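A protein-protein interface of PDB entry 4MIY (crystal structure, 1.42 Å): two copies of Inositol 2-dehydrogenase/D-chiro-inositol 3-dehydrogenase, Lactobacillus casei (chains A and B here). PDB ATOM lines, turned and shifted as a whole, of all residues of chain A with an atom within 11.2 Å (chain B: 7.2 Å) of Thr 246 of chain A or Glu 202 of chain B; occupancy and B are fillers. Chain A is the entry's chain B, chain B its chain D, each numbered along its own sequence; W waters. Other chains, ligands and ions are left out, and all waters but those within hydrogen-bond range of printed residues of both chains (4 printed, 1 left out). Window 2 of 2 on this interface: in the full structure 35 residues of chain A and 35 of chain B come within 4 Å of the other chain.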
ATOM      1  N   LYS A 139       5.386 -22.278  -7.367  1.00  0.00           N
ATOM      2  CA  LYS A 139       4.980 -22.029  -8.730  1.00  0.00           C
ATOM      3  C   LYS A 139       3.568 -22.576  -8.976  1.00  0.00           C
ATOM      4  O   LYS A 139       2.789 -21.957  -9.633  1.00  0.00           O
ATOM      5  CB  LYS A 139       6.002 -22.616  -9.702  1.00  0.00           C
ATOM      6  CG  LYS A 139       5.811 -22.254 -11.144  1.00  0.00           C
ATOM      7  CD  LYS A 139       6.106 -20.803 -11.377  1.00  0.00           C
ATOM      8  CE  LYS A 139       6.231 -20.476 -12.842  1.00  0.00           C
ATOM      9  NZ  LYS A 139       6.424 -19.040 -13.028  1.00  0.00           N
ATOM     10  N   LEU A 140       3.268 -23.727  -8.411  1.00  0.00           N
ATOM     11  CA  LEU A 140       1.934 -24.280  -8.485  1.00  0.00           C
ATOM     12  C   LEU A 140       0.879 -23.303  -7.952  1.00  0.00           C
ATOM     13  O   LEU A 140      -0.129 -23.080  -8.533  1.00  0.00           O
ATOM     14  CB  LEU A 140       1.886 -25.602  -7.713  1.00  0.00           C
ATOM     15  CG  LEU A 140       0.547 -26.288  -7.626  1.00  0.00           C
ATOM     16  CD1 LEU A 140      -0.007 -26.631  -8.970  1.00  0.00           C
ATOM     17  CD2 LEU A 140       0.662 -27.494  -6.750  1.00  0.00           C
ATOM     18  N   THR A 142       0.817 -20.183  -7.844  1.00  0.00           N
ATOM     19  CA  THR A 142       0.583 -19.018  -8.699  1.00  0.00           C
ATOM     20  C   THR A 142      -0.598 -19.187  -9.632  1.00  0.00           C
ATOM     21  O   THR A 142      -1.084 -18.260 -10.173  1.00  0.00           O
ATOM     22  CB  THR A 142       1.777 -18.626  -9.572  1.00  0.00           C
ATOM     23  OG1 THR A 142       2.004 -19.618 -10.552  1.00  0.00           O
ATOM     24  CG2 THR A 142       3.040 -18.403  -8.791  1.00  0.00           C
ATOM     25  N   GLY A 143      -1.021 -20.414  -9.816  1.00  0.00           N
ATOM     26  CA  GLY A 143      -2.082 -20.734 -10.726  1.00  0.00           C
ATOM     27  C   GLY A 143      -1.703 -20.958 -12.175  1.00  0.00           C
ATOM     28  O   GLY A 143      -2.548 -21.183 -12.980  1.00  0.00           O
ATOM     29  N   ILE A 144      -0.429 -20.902 -12.464  1.00  0.00           N
ATOM     30  CA  ILE A 144       0.064 -20.907 -13.829  1.00  0.00           C
ATOM     31  C   ILE A 144      -0.218 -22.186 -14.644  1.00  0.00           C
ATOM     32  O   ILE A 144      -0.316 -22.132 -15.815  1.00  0.00           O
ATOM     33  CB  ILE A 144       1.556 -20.524 -13.862  1.00  0.00           C
ATOM     34  CG1 ILE A 144       2.007 -20.195 -15.276  1.00  0.00           C
ATOM     35  CG2 ILE A 144       2.410 -21.586 -13.252  1.00  0.00           C
ATOM     36  CD1 ILE A 144       3.300 -19.456 -15.303  1.00  0.00           C
ATOM     37  N   ILE A 145      -0.372 -23.300 -13.968  1.00  0.00           N
ATOM     38  CA  ILE A 145      -0.785 -24.522 -14.623  1.00  0.00           C
ATOM     39  C   ILE A 145      -2.192 -24.944 -14.295  1.00  0.00           C
ATOM     40  O   ILE A 145      -2.601 -26.004 -14.615  1.00  0.00           O
ATOM     41  CB  ILE A 145       0.220 -25.699 -14.403  1.00  0.00           C
ATOM     42  CG1 ILE A 145       0.271 -26.167 -12.955  1.00  0.00           C
ATOM     43  CG2 ILE A 145       1.561 -25.288 -14.816  1.00  0.00           C
ATOM     44  CD1 ILE A 145       0.992 -27.465 -12.803  1.00  0.00           C
ATOM     45  N   GLY A 146      -2.948 -24.039 -13.707  1.00  0.00           N
ATOM     46  CA  GLY A 146      -4.273 -24.373 -13.275  1.00  0.00           C
ATOM     47  C   GLY A 146      -4.288 -25.351 -12.118  1.00  0.00           C
ATOM     48  O   GLY A 146      -3.354 -25.480 -11.413  1.00  0.00           O
ATOM     49  N   ALA A 147      -5.405 -26.018 -11.948  1.00  0.00           N
ATOM     50  CA  ALA A 147      -5.561 -26.922 -10.839  1.00  0.00           C
ATOM     51  C   ALA A 147      -4.781 -28.228 -11.027  1.00  0.00           C
ATOM     52  O   ALA A 147      -4.698 -28.747 -12.080  1.00  0.00           O
ATOM     53  CB  ALA A 147      -7.015 -27.196 -10.588  1.00  0.00           C
ATOM     54  N   PRO A 148      -4.220 -28.742  -9.952  1.00  0.00           N
ATOM     55  CA  PRO A 148      -3.495 -30.002 -10.032  1.00  0.00           C
ATOM     56  C   PRO A 148      -4.434 -31.212 -10.113  1.00  0.00           C
ATOM     57  O   PRO A 148      -5.263 -31.391  -9.276  1.00  0.00           O
ATOM     58  CB  PRO A 148      -2.683 -30.016  -8.734  1.00  0.00           C
ATOM     59  CG  PRO A 148      -3.496 -29.228  -7.806  1.00  0.00           C
ATOM     60  CD  PRO A 148      -4.130 -28.149  -8.616  1.00  0.00           C
ATOM     61  N   LEU A 149      -4.247 -32.006 -11.146  1.00  0.00           N
ATOM     62  CA  LEU A 149      -5.102 -33.134 -11.443  1.00  0.00           C
ATOM     63  C   LEU A 149      -4.477 -34.448 -11.064  1.00  0.00           C
ATOM     64  O   LEU A 149      -5.135 -35.294 -10.573  1.00  0.00           O
ATOM     65  CB  LEU A 149      -5.462 -33.124 -12.917  1.00  0.00           C
ATOM     66  CG  LEU A 149      -6.019 -31.815 -13.469  1.00  0.00           C
ATOM     67  CD1 LEU A 149      -6.244 -31.854 -14.944  1.00  0.00           C
ATOM     68  CD2 LEU A 149      -7.287 -31.411 -12.769  1.00  0.00           C
ATOM     69  N   VAL A 150      -3.209 -34.593 -11.353  1.00  0.00           N
ATOM     70  CA  VAL A 150      -2.462 -35.794 -11.092  1.00  0.00           C
ATOM     71  C   VAL A 150      -1.072 -35.373 -10.601  1.00  0.00           C
ATOM     72  O   VAL A 150      -0.520 -34.397 -11.038  1.00  0.00           O
ATOM     73  CB  VAL A 150      -2.327 -36.648 -12.367  1.00  0.00           C
ATOM     74  CG1 VAL A 150      -1.463 -37.851 -12.143  1.00  0.00           C
ATOM     75  CG2 VAL A 150      -3.649 -37.110 -12.867  1.00  0.00           C
ATOM     76  N   VAL A 242       3.832 -32.491 -11.294  1.00  0.00           N
ATOM     77  CA  VAL A 242       2.460 -32.127 -11.095  1.00  0.00           C
ATOM     78  C   VAL A 242       1.813 -31.813 -12.446  1.00  0.00           C
ATOM     79  O   VAL A 242       2.289 -31.017 -13.190  1.00  0.00           O
ATOM     80  CB  VAL A 242       2.302 -30.916 -10.113  1.00  0.00           C
ATOM     81  CG1 VAL A 242       0.863 -30.594  -9.937  1.00  0.00           C
ATOM     82  CG2 VAL A 242       2.914 -31.236  -8.766  1.00  0.00           C
ATOM     83  N   ILE A 243       0.752 -32.531 -12.734  1.00  0.00           N
ATOM     84  CA  ILE A 243      -0.033 -32.364 -13.944  1.00  0.00           C
ATOM     85  C   ILE A 243      -1.226 -31.441 -13.671  1.00  0.00           C
ATOM     86  O   ILE A 243      -2.104 -31.767 -12.938  1.00  0.00           O
ATOM     87  CB  ILE A 243      -0.609 -33.711 -14.381  1.00  0.00           C
ATOM     88  CG1 ILE A 243       0.469 -34.786 -14.487  1.00  0.00           C
ATOM     89  CG2 ILE A 243      -1.372 -33.570 -15.658  1.00  0.00           C
ATOM     90  CD1 ILE A 243       1.520 -34.482 -15.394  1.00  0.00           C
ATOM     91  N   GLY A 244      -1.207 -30.294 -14.307  1.00  0.00           N
ATOM     92  CA  GLY A 244      -2.265 -29.340 -14.176  1.00  0.00           C
ATOM     93  C   GLY A 244      -3.171 -29.248 -15.373  1.00  0.00           C
ATOM     94  O   GLY A 244      -2.902 -29.804 -16.380  1.00  0.00           O
ATOM     95  N   GLU A 245      -4.226 -28.486 -15.206  1.00  0.00           N
ATOM     96  CA  GLU A 245      -5.176 -28.258 -16.261  1.00  0.00           C
ATOM     97  C   GLU A 245      -4.550 -27.684 -17.523  1.00  0.00           C
ATOM     98  O   GLU A 245      -4.916 -28.047 -18.580  1.00  0.00           O
ATOM     99  CB  GLU A 245      -6.298 -27.352 -15.775  1.00  0.00           C
ATOM    100  CG  GLU A 245      -7.205 -27.997 -14.758  1.00  0.00           C
ATOM    101  CD  GLU A 245      -8.161 -27.030 -14.074  1.00  0.00           C
ATOM    102  OE1 GLU A 245      -7.755 -25.922 -13.762  1.00  0.00           O
ATOM    103  OE2 GLU A 245      -9.294 -27.445 -13.835  1.00  0.00           O
ATOM    104  N   THR A 246      -3.599 -26.779 -17.357  1.00  0.00           N
ATOM    105  CA  THR A 246      -3.048 -26.036 -18.476  1.00  0.00           C
ATOM    106  C   THR A 246      -1.540 -26.131 -18.625  1.00  0.00           C
ATOM    107  O   THR A 246      -0.961 -25.502 -19.453  1.00  0.00           O
ATOM    108  CB  THR A 246      -3.421 -24.543 -18.387  1.00  0.00           C
ATOM    109  OG1 THR A 246      -2.735 -23.948 -17.295  1.00  0.00           O
ATOM    110  CG2 THR A 246      -4.898 -24.349 -18.222  1.00  0.00           C
ATOM    111  N   GLY A 247      -0.921 -26.933 -17.784  1.00  0.00           N
ATOM    112  CA  GLY A 247       0.485 -27.157 -17.892  1.00  0.00           C
ATOM    113  C   GLY A 247       0.997 -28.161 -16.900  1.00  0.00           C
ATOM    114  O   GLY A 247       0.221 -28.761 -16.214  1.00  0.00           O
ATOM    115  N   GLU A 248       2.309 -28.312 -16.849  1.00  0.00           N
ATOM    116  CA  GLU A 248       2.947 -29.232 -15.914  1.00  0.00           C
ATOM    117  C   GLU A 248       4.132 -28.583 -15.216  1.00  0.00           C
ATOM    118  O   GLU A 248       4.737 -27.690 -15.745  1.00  0.00           O
ATOM    119  CB  GLU A 248       3.430 -30.520 -16.609  1.00  0.00           C
ATOM    120  CG  GLU A 248       2.387 -31.300 -17.391  1.00  0.00           C
ATOM    121  CD  GLU A 248       2.966 -32.598 -17.958  1.00  0.00           C
ATOM    122  OE1 GLU A 248       4.155 -32.804 -17.816  1.00  0.00           O
ATOM    123  OE2 GLU A 248       2.205 -33.362 -18.555  1.00  0.00           O
ATOM    124  N   LEU A 249       4.443 -29.092 -14.030  1.00  0.00           N
ATOM    125  CA  LEU A 249       5.621 -28.697 -13.268  1.00  0.00           C
ATOM    126  C   LEU A 249       6.408 -29.931 -12.806  1.00  0.00           C
ATOM    127  O   LEU A 249       5.834 -30.865 -12.370  1.00  0.00           O
ATOM    128  CB  LEU A 249       5.211 -27.874 -12.050  1.00  0.00           C
ATOM    129  CG  LEU A 249       4.720 -26.456 -12.290  1.00  0.00           C
ATOM    130  CD1 LEU A 249       4.053 -25.922 -11.073  1.00  0.00           C
ATOM    131  CD2 LEU A 249       5.846 -25.590 -12.673  1.00  0.00           C
ATOM    132  N   PRO B 158      -2.709 -31.194 -26.701  1.00  0.00           N
ATOM    133  CA  PRO B 158      -3.100 -29.883 -26.197  1.00  0.00           C
ATOM    134  C   PRO B 158      -4.614 -29.684 -26.109  1.00  0.00           C
ATOM    135  O   PRO B 158      -5.099 -29.094 -25.195  1.00  0.00           O
ATOM    136  CB  PRO B 158      -2.498 -28.933 -27.219  1.00  0.00           C
ATOM    137  CG  PRO B 158      -2.221 -29.736 -28.388  1.00  0.00           C
ATOM    138  CD  PRO B 158      -1.949 -31.095 -27.945  1.00  0.00           C
ATOM    139  N   ASN B 159      -5.313 -30.203 -27.091  1.00  0.00           N
ATOM    140  CA  ASN B 159      -6.755 -30.097 -27.173  1.00  0.00           C
ATOM    141  C   ASN B 159      -7.306 -31.134 -28.144  1.00  0.00           C
ATOM    142  O   ASN B 159      -6.566 -31.731 -28.838  1.00  0.00           O
ATOM    143  CB  ASN B 159      -7.201 -28.707 -27.616  1.00  0.00           C
ATOM    144  CG  ASN B 159      -7.351 -27.750 -26.483  1.00  0.00           C
ATOM    145  OD1 ASN B 159      -8.081 -27.998 -25.540  1.00  0.00           O
ATOM    146  ND2 ASN B 159      -6.635 -26.638 -26.557  1.00  0.00           N
ATOM    147  N   GLN B 199     -11.512 -34.033 -12.793  1.00  0.00           N
ATOM    148  CA  GLN B 199     -11.897 -33.590 -14.129  1.00  0.00           C
ATOM    149  C   GLN B 199     -11.375 -32.191 -14.445  1.00  0.00           C
ATOM    150  O   GLN B 199     -11.544 -31.295 -13.705  1.00  0.00           O
ATOM    151  CB  GLN B 199     -13.414 -33.641 -14.298  1.00  0.00           C
ATOM    152  CG  GLN B 199     -13.942 -33.076 -15.595  1.00  0.00           C
ATOM    153  CD  GLN B 199     -13.801 -34.022 -16.787  1.00  0.00           C
ATOM    154  OE1 GLN B 199     -13.141 -35.011 -16.734  1.00  0.00           O
ATOM    155  NE2 GLN B 199     -14.427 -33.663 -17.864  1.00  0.00           N
ATOM    156  N   SER B 200     -10.722 -32.050 -15.580  1.00  0.00           N
ATOM    157  CA  SER B 200     -10.208 -30.764 -15.984  1.00  0.00           C
ATOM    158  C   SER B 200     -11.303 -29.793 -16.384  1.00  0.00           C
ATOM    159  O   SER B 200     -12.203 -30.132 -17.073  1.00  0.00           O
ATOM    160  CB  SER B 200      -9.279 -30.922 -17.176  1.00  0.00           C
ATOM    161  OG  SER B 200      -8.728 -29.701 -17.521  1.00  0.00           O
ATOM    162  N   ALA B 201     -11.129 -28.556 -15.976  1.00  0.00           N
ATOM    163  CA  ALA B 201     -11.987 -27.486 -16.429  1.00  0.00           C
ATOM    164  C   ALA B 201     -11.816 -27.179 -17.905  1.00  0.00           C
ATOM    165  O   ALA B 201     -12.572 -26.436 -18.442  1.00  0.00           O
ATOM    166  CB  ALA B 201     -11.714 -26.227 -15.612  1.00  0.00           C
ATOM    167  N   GLU B 202     -10.791 -27.751 -18.533  1.00  0.00           N
ATOM    168  CA  GLU B 202     -10.496 -27.474 -19.932  1.00  0.00           C
ATOM    169  C   GLU B 202     -11.285 -28.325 -20.940  1.00  0.00           C
ATOM    170  O   GLU B 202     -11.285 -28.050 -22.114  1.00  0.00           O
ATOM    171  CB  GLU B 202      -8.998 -27.564 -20.228  1.00  0.00           C
ATOM    172  CG  GLU B 202      -8.139 -26.607 -19.443  1.00  0.00           C
ATOM    173  CD  GLU B 202      -8.457 -25.140 -19.676  1.00  0.00           C
ATOM    174  OE1 GLU B 202      -8.552 -24.406 -18.704  1.00  0.00           O
ATOM    175  OE2 GLU B 202      -8.595 -24.728 -20.815  1.00  0.00           O
ATOM    176  N   VAL B 203     -11.973 -29.326 -20.433  1.00  0.00           N
ATOM    177  CA  VAL B 203     -12.782 -30.186 -21.258  1.00  0.00           C
ATOM    178  C   VAL B 203     -13.943 -29.422 -21.870  1.00  0.00           C
ATOM    179  O   VAL B 203     -14.621 -28.702 -21.193  1.00  0.00           O
ATOM    180  CB  VAL B 203     -13.284 -31.342 -20.459  1.00  0.00           C
ATOM    181  CG1 VAL B 203     -14.322 -32.127 -21.242  1.00  0.00           C
ATOM    182  CG2 VAL B 203     -12.136 -32.226 -20.086  1.00  0.00           C
ATOM    183  N   ARG B 204     -14.152 -29.614 -23.149  1.00  0.00           N
ATOM    184  CA  ARG B 204     -15.215 -28.937 -23.868  1.00  0.00           C
ATOM    185  C   ARG B 204     -16.164 -29.870 -24.579  1.00  0.00           C
ATOM    186  O   ARG B 204     -17.001 -29.436 -25.309  1.00  0.00           O
ATOM    187  CB  ARG B 204     -14.619 -28.004 -24.900  1.00  0.00           C
ATOM    188  CG  ARG B 204     -13.839 -26.899 -24.293  1.00  0.00           C
ATOM    189  CD  ARG B 204     -12.926 -26.334 -25.275  1.00  0.00           C
ATOM    190  NE  ARG B 204     -13.506 -26.423 -26.598  1.00  0.00           N
ATOM    191  CZ  ARG B 204     -14.209 -25.469 -27.164  1.00  0.00           C
ATOM    192  NH1 ARG B 204     -14.423 -24.336 -26.531  1.00  0.00           N
ATOM    193  NH2 ARG B 204     -14.692 -25.666 -28.360  1.00  0.00           N
ATOM    194  N   ASN B 205     -15.964 -31.147 -24.379  1.00  0.00           N
ATOM    195  CA  ASN B 205     -16.712 -32.162 -25.074  1.00  0.00           C
ATOM    196  C   ASN B 205     -17.559 -32.942 -24.084  1.00  0.00           C
ATOM    197  O   ASN B 205     -17.054 -33.478 -23.151  1.00  0.00           O
ATOM    198  CB  ASN B 205     -15.763 -33.141 -25.779  1.00  0.00           C
ATOM    199  CG  ASN B 205     -14.945 -32.509 -26.879  1.00  0.00           C
ATOM    200  OD1 ASN B 205     -14.627 -31.356 -26.855  1.00  0.00           O
ATOM    201  ND2 ASN B 205     -14.570 -33.316 -27.820  1.00  0.00           N
ATOM    202  N   ASP B 210     -11.242 -36.301 -18.691  1.00  0.00           N
ATOM    203  CA  ASP B 210      -9.870 -35.965 -18.958  1.00  0.00           C
ATOM    204  C   ASP B 210      -9.316 -35.248 -17.752  1.00  0.00           C
ATOM    205  O   ASP B 210      -9.914 -34.354 -17.264  1.00  0.00           O
ATOM    206  CB  ASP B 210      -9.741 -35.079 -20.194  1.00  0.00           C
ATOM    207  CG  ASP B 210      -8.294 -34.921 -20.672  1.00  0.00           C
ATOM    208  OD1 ASP B 210      -7.641 -35.928 -20.920  1.00  0.00           O
ATOM    209  OD2 ASP B 210      -7.853 -33.801 -20.808  1.00  0.00           O
ATOM    210  N   HIS B 229      -3.783 -37.402 -21.305  1.00  0.00           N
ATOM    211  CA  HIS B 229      -4.227 -36.049 -21.001  1.00  0.00           C
ATOM    212  C   HIS B 229      -4.348 -35.300 -22.302  1.00  0.00           C
ATOM    213  O   HIS B 229      -3.394 -34.847 -22.829  1.00  0.00           O
ATOM    214  CB  HIS B 229      -3.256 -35.350 -20.065  1.00  0.00           C
ATOM    215  CG  HIS B 229      -3.785 -34.086 -19.473  1.00  0.00           C
ATOM    216  ND1 HIS B 229      -2.991 -33.221 -18.771  1.00  0.00           N
ATOM    217  CD2 HIS B 229      -5.015 -33.544 -19.480  1.00  0.00           C
ATOM    218  CE1 HIS B 229      -3.717 -32.204 -18.370  1.00  0.00           C
ATOM    219  NE2 HIS B 229      -4.940 -32.364 -18.808  1.00  0.00           N
ATOM    220  N   THR B 231      -6.470 -32.581 -23.067  1.00  0.00           N
ATOM    221  CA  THR B 231      -6.773 -31.163 -23.030  1.00  0.00           C
ATOM    222  C   THR B 231      -5.707 -30.411 -22.249  1.00  0.00           C
ATOM    223  O   THR B 231      -5.983 -29.449 -21.592  1.00  0.00           O
ATOM    224  CB  THR B 231      -8.147 -30.845 -22.436  1.00  0.00           C
ATOM    225  OG1 THR B 231      -8.212 -31.241 -21.070  1.00  0.00           O
ATOM    226  CG2 THR B 231      -9.224 -31.540 -23.219  1.00  0.00           C
ATOM    227  N   ALA B 232      -4.479 -30.870 -22.367  1.00  0.00           N
ATOM    228  CA  ALA B 232      -3.375 -30.353 -21.575  1.00  0.00           C
ATOM    229  C   ALA B 232      -2.953 -28.921 -21.841  1.00  0.00           C
ATOM    230  O   ALA B 232      -2.262 -28.368 -21.061  1.00  0.00           O
ATOM    231  CB  ALA B 232      -2.204 -31.259 -21.697  1.00  0.00           C
ATOM    232  N   GLN B 233      -3.375 -28.380 -22.966  1.00  0.00           N
ATOM    233  CA  GLN B 233      -3.126 -26.997 -23.422  1.00  0.00           C
ATOM    234  C   GLN B 233      -1.707 -26.684 -23.903  1.00  0.00           C
ATOM    235  O   GLN B 233      -1.526 -26.042 -24.894  1.00  0.00           O
ATOM    236  CB  GLN B 233      -3.576 -25.953 -22.399  1.00  0.00           C
ATOM    237  CG  GLN B 233      -5.002 -26.083 -21.917  1.00  0.00           C
ATOM    238  CD  GLN B 233      -6.011 -26.060 -23.034  1.00  0.00           C
ATOM    239  OE1 GLN B 233      -6.052 -25.146 -23.777  1.00  0.00           O
ATOM    240  NE2 GLN B 233      -6.822 -27.093 -23.129  1.00  0.00           N
ATOM    241  N   TYR B 234      -0.714 -27.156 -23.172  1.00  0.00           N
ATOM    242  CA  TYR B 234       0.636 -26.671 -23.359  1.00  0.00           C
ATOM    243  C   TYR B 234       1.326 -27.188 -24.601  1.00  0.00           C
ATOM    244  O   TYR B 234       2.172 -26.568 -25.107  1.00  0.00           O
ATOM    245  CB  TYR B 234       1.526 -26.955 -22.119  1.00  0.00           C
ATOM    246  CG  TYR B 234       2.092 -28.374 -22.000  1.00  0.00           C
ATOM    247  CD1 TYR B 234       3.254 -28.745 -22.635  1.00  0.00           C
ATOM    248  CD2 TYR B 234       1.459 -29.319 -21.254  1.00  0.00           C
ATOM    249  CE1 TYR B 234       3.746 -30.022 -22.538  1.00  0.00           C
ATOM    250  CE2 TYR B 234       1.950 -30.575 -21.163  1.00  0.00           C
ATOM    251  CZ  TYR B 234       3.079 -30.918 -21.801  1.00  0.00           C
ATOM    252  OH  TYR B 234       3.558 -32.191 -21.688  1.00  0.00           O
ATOM    253  N   GLY B 235       0.935 -28.363 -25.049  1.00  0.00           N
ATOM    254  CA  GLY B 235       1.646 -28.988 -26.122  1.00  0.00           C
ATOM    255  C   GLY B 235       1.261 -30.438 -26.330  1.00  0.00           C
ATOM    256  O   GLY B 235       0.400 -30.948 -25.682  1.00  0.00           O
HETATM  257  O   HOH W   1      -0.257 -32.571 -18.927  1.00  0.00           O
HETATM  258  O   HOH W   2     -10.511 -29.273 -12.231  1.00  0.00           O
HETATM  259  O   HOH W   3      -7.620 -24.026 -15.814  1.00  0.00           O
HETATM  260  O   HOH W   4      -6.583 -30.161 -18.995  1.00  0.00           O
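Water W1 bridges OE2 of Glu 248 of chain A and ND1 of His 229 of chain B. Water W4 lies within hydrogen-bond range of the side-chain hydroxyl of Ser 200 of chain B (2.6 Å), the backbone carbonyl oxygen of Glu 245 of chain A (2.7 Å), a ring nitrogen (NE2) of His 229 of chain B (2.8 Å) and the backbone carbonyl oxygen of Thr 231 of chain B (2.8 Å). Water W2 bridges the backbone carbonyl oxygen of Gln 199 of chain B and the side-chain carboxylate of Glu 245 of chain A. Water W3 bridges the side-chain carboxylate (OE1) of Glu 245 of chain A (2.8 Å) and the side-chain carboxylate (OE1) of Glu 202 of chain B (3.1 Å).
OG1 of Thr 246 of chain A sits at hydrogen-bond distance from O of Ile 144 of chain A (3.4 Å). The backbone carbonyl oxygen (O) of Ile 243 of chain A sits at hydrogen-bond distance from the backbone NH (N) of Leu 149 of chain A (2.8 Å). The side-chain amide oxygen (OD1) of Asn 159 of chain B sits at hydrogen-bond distance from the side-chain amide nitrogen (NE2) of Gln 233 of chain B (2.9 Å). The backbone NH (N) of Ser 200 of chain B lies within hydrogen-bond range of the backbone carbonyl oxygen (O) of Asp 210 of chain B, at 3.0 Å. The side-chain hydroxyl (OG1) of Thr 231 of chain B sits at hydrogen-bond distance from the side-chain carboxylate (OD2) of Asp 210 of chain B (2.6 Å). The side-chain amide nitrogen (NE2) of Gln 233 of chain B is in hydrogen-bond range of the backbone carbonyl oxygen (O) of Thr 231 of chain B, 2.9 Å away.
Printed residues of chain B within 4 Å of Thr 246 of chain A: Glu 202, Ala 232, Gln 233 and Tyr 234. Glu 202 of chain B touches just these residues of chain A: Glu 245 and Thr 246. No residue of chain A comes within 4 Å of Val 203 of chain B. Thr 231 of chain B touches just one residue of chain A: Glu 245 (3.5 Å). Of chain A, only Glu 245 (3.6 Å), Thr 246 (3.4 Å) and Gly 247 (3.8 Å) come within 4 Å of Ala 232 of chain B. Gln 233 of chain B touches just these residues of chain A: Glu 245 (3.9 Å) and Thr 246 (3.96 Å). Of the printed residues of chain B, Glu 245 of chain A touches Ser 200, Ala 201, Glu 202, Thr 231, Ala 232 and Gln 233. Of the printed residues of chain B, Gly 244 of chain A touches His 229 (3.2 Å). Of the printed residues of chain B, Glu 248 of chain A touches Tyr 234. Printed residues of chain B within 4 Å of Leu 149 of chain A: Ser 200. The nearest residue of chain B that does not touch Thr 246 of chain A is Thr 231 of chain B (5.5 Å). The nearest residue of chain A that does not touch Glu 202 of chain B is Gly 244 of chain A (6.9 Å). The nearest printed residue of chain B that does not touch Ile 243 of chain A is Ala 232 of chain B (6.5 Å).
Among the printed residues, merely in contact across the chains: Gly 244 of chain A with His 229 of chain B (3.2 Å), Thr 246 of chain A with Ala 232 of chain B (3.4 Å), Ile 243 of chain A with His 229 of chain B (3.5 Å), Glu 245 of chain A with Ser 200 of chain B (3.6 Å), Glu 248 of chain A with Tyr 234 of chain B (3.6 Å), Glu 245 of chain A with Glu 202 of chain B (3.6 Å), Glu 245 of chain A with Ala 232 of chain B (3.6 Å), Thr 246 of chain A with Glu 202 of chain B (3.7 Å), Gly 247 of chain A with Ala 232 of chain B (3.8 Å), Glu 245 of chain A with Gln 233 of chain B (3.9 Å), Leu 149 of chain A with Ser 200 of chain B (3.9 Å), Thr 246 of chain A with Tyr 234 of chain B (3.9 Å) and Thr 246 of chain A with Gln 233 of chain B (3.96 Å).
No position is printed for both chains.
Of the 16 printed residues of chain B, 8 touch a printed residue of chain A. Printed residues of chain B that touch a printed residue of chain A: Ser 200, Ala 201, Glu 202, His 229, Thr 231, Ala 232, Gln 233 and Tyr 234. Printed residues of chain A that touch a printed residue of chain B: Leu 149, Ile 243, Gly 244, Glu 245, Thr 246, Gly 247 and Glu 248.
OE2 of Glu 245 of chain A sits at hydrogen-bond distance from N of Ala 201 of chain B. O of Glu 245 of chain A sits close to O of Thr 231 of chain B.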
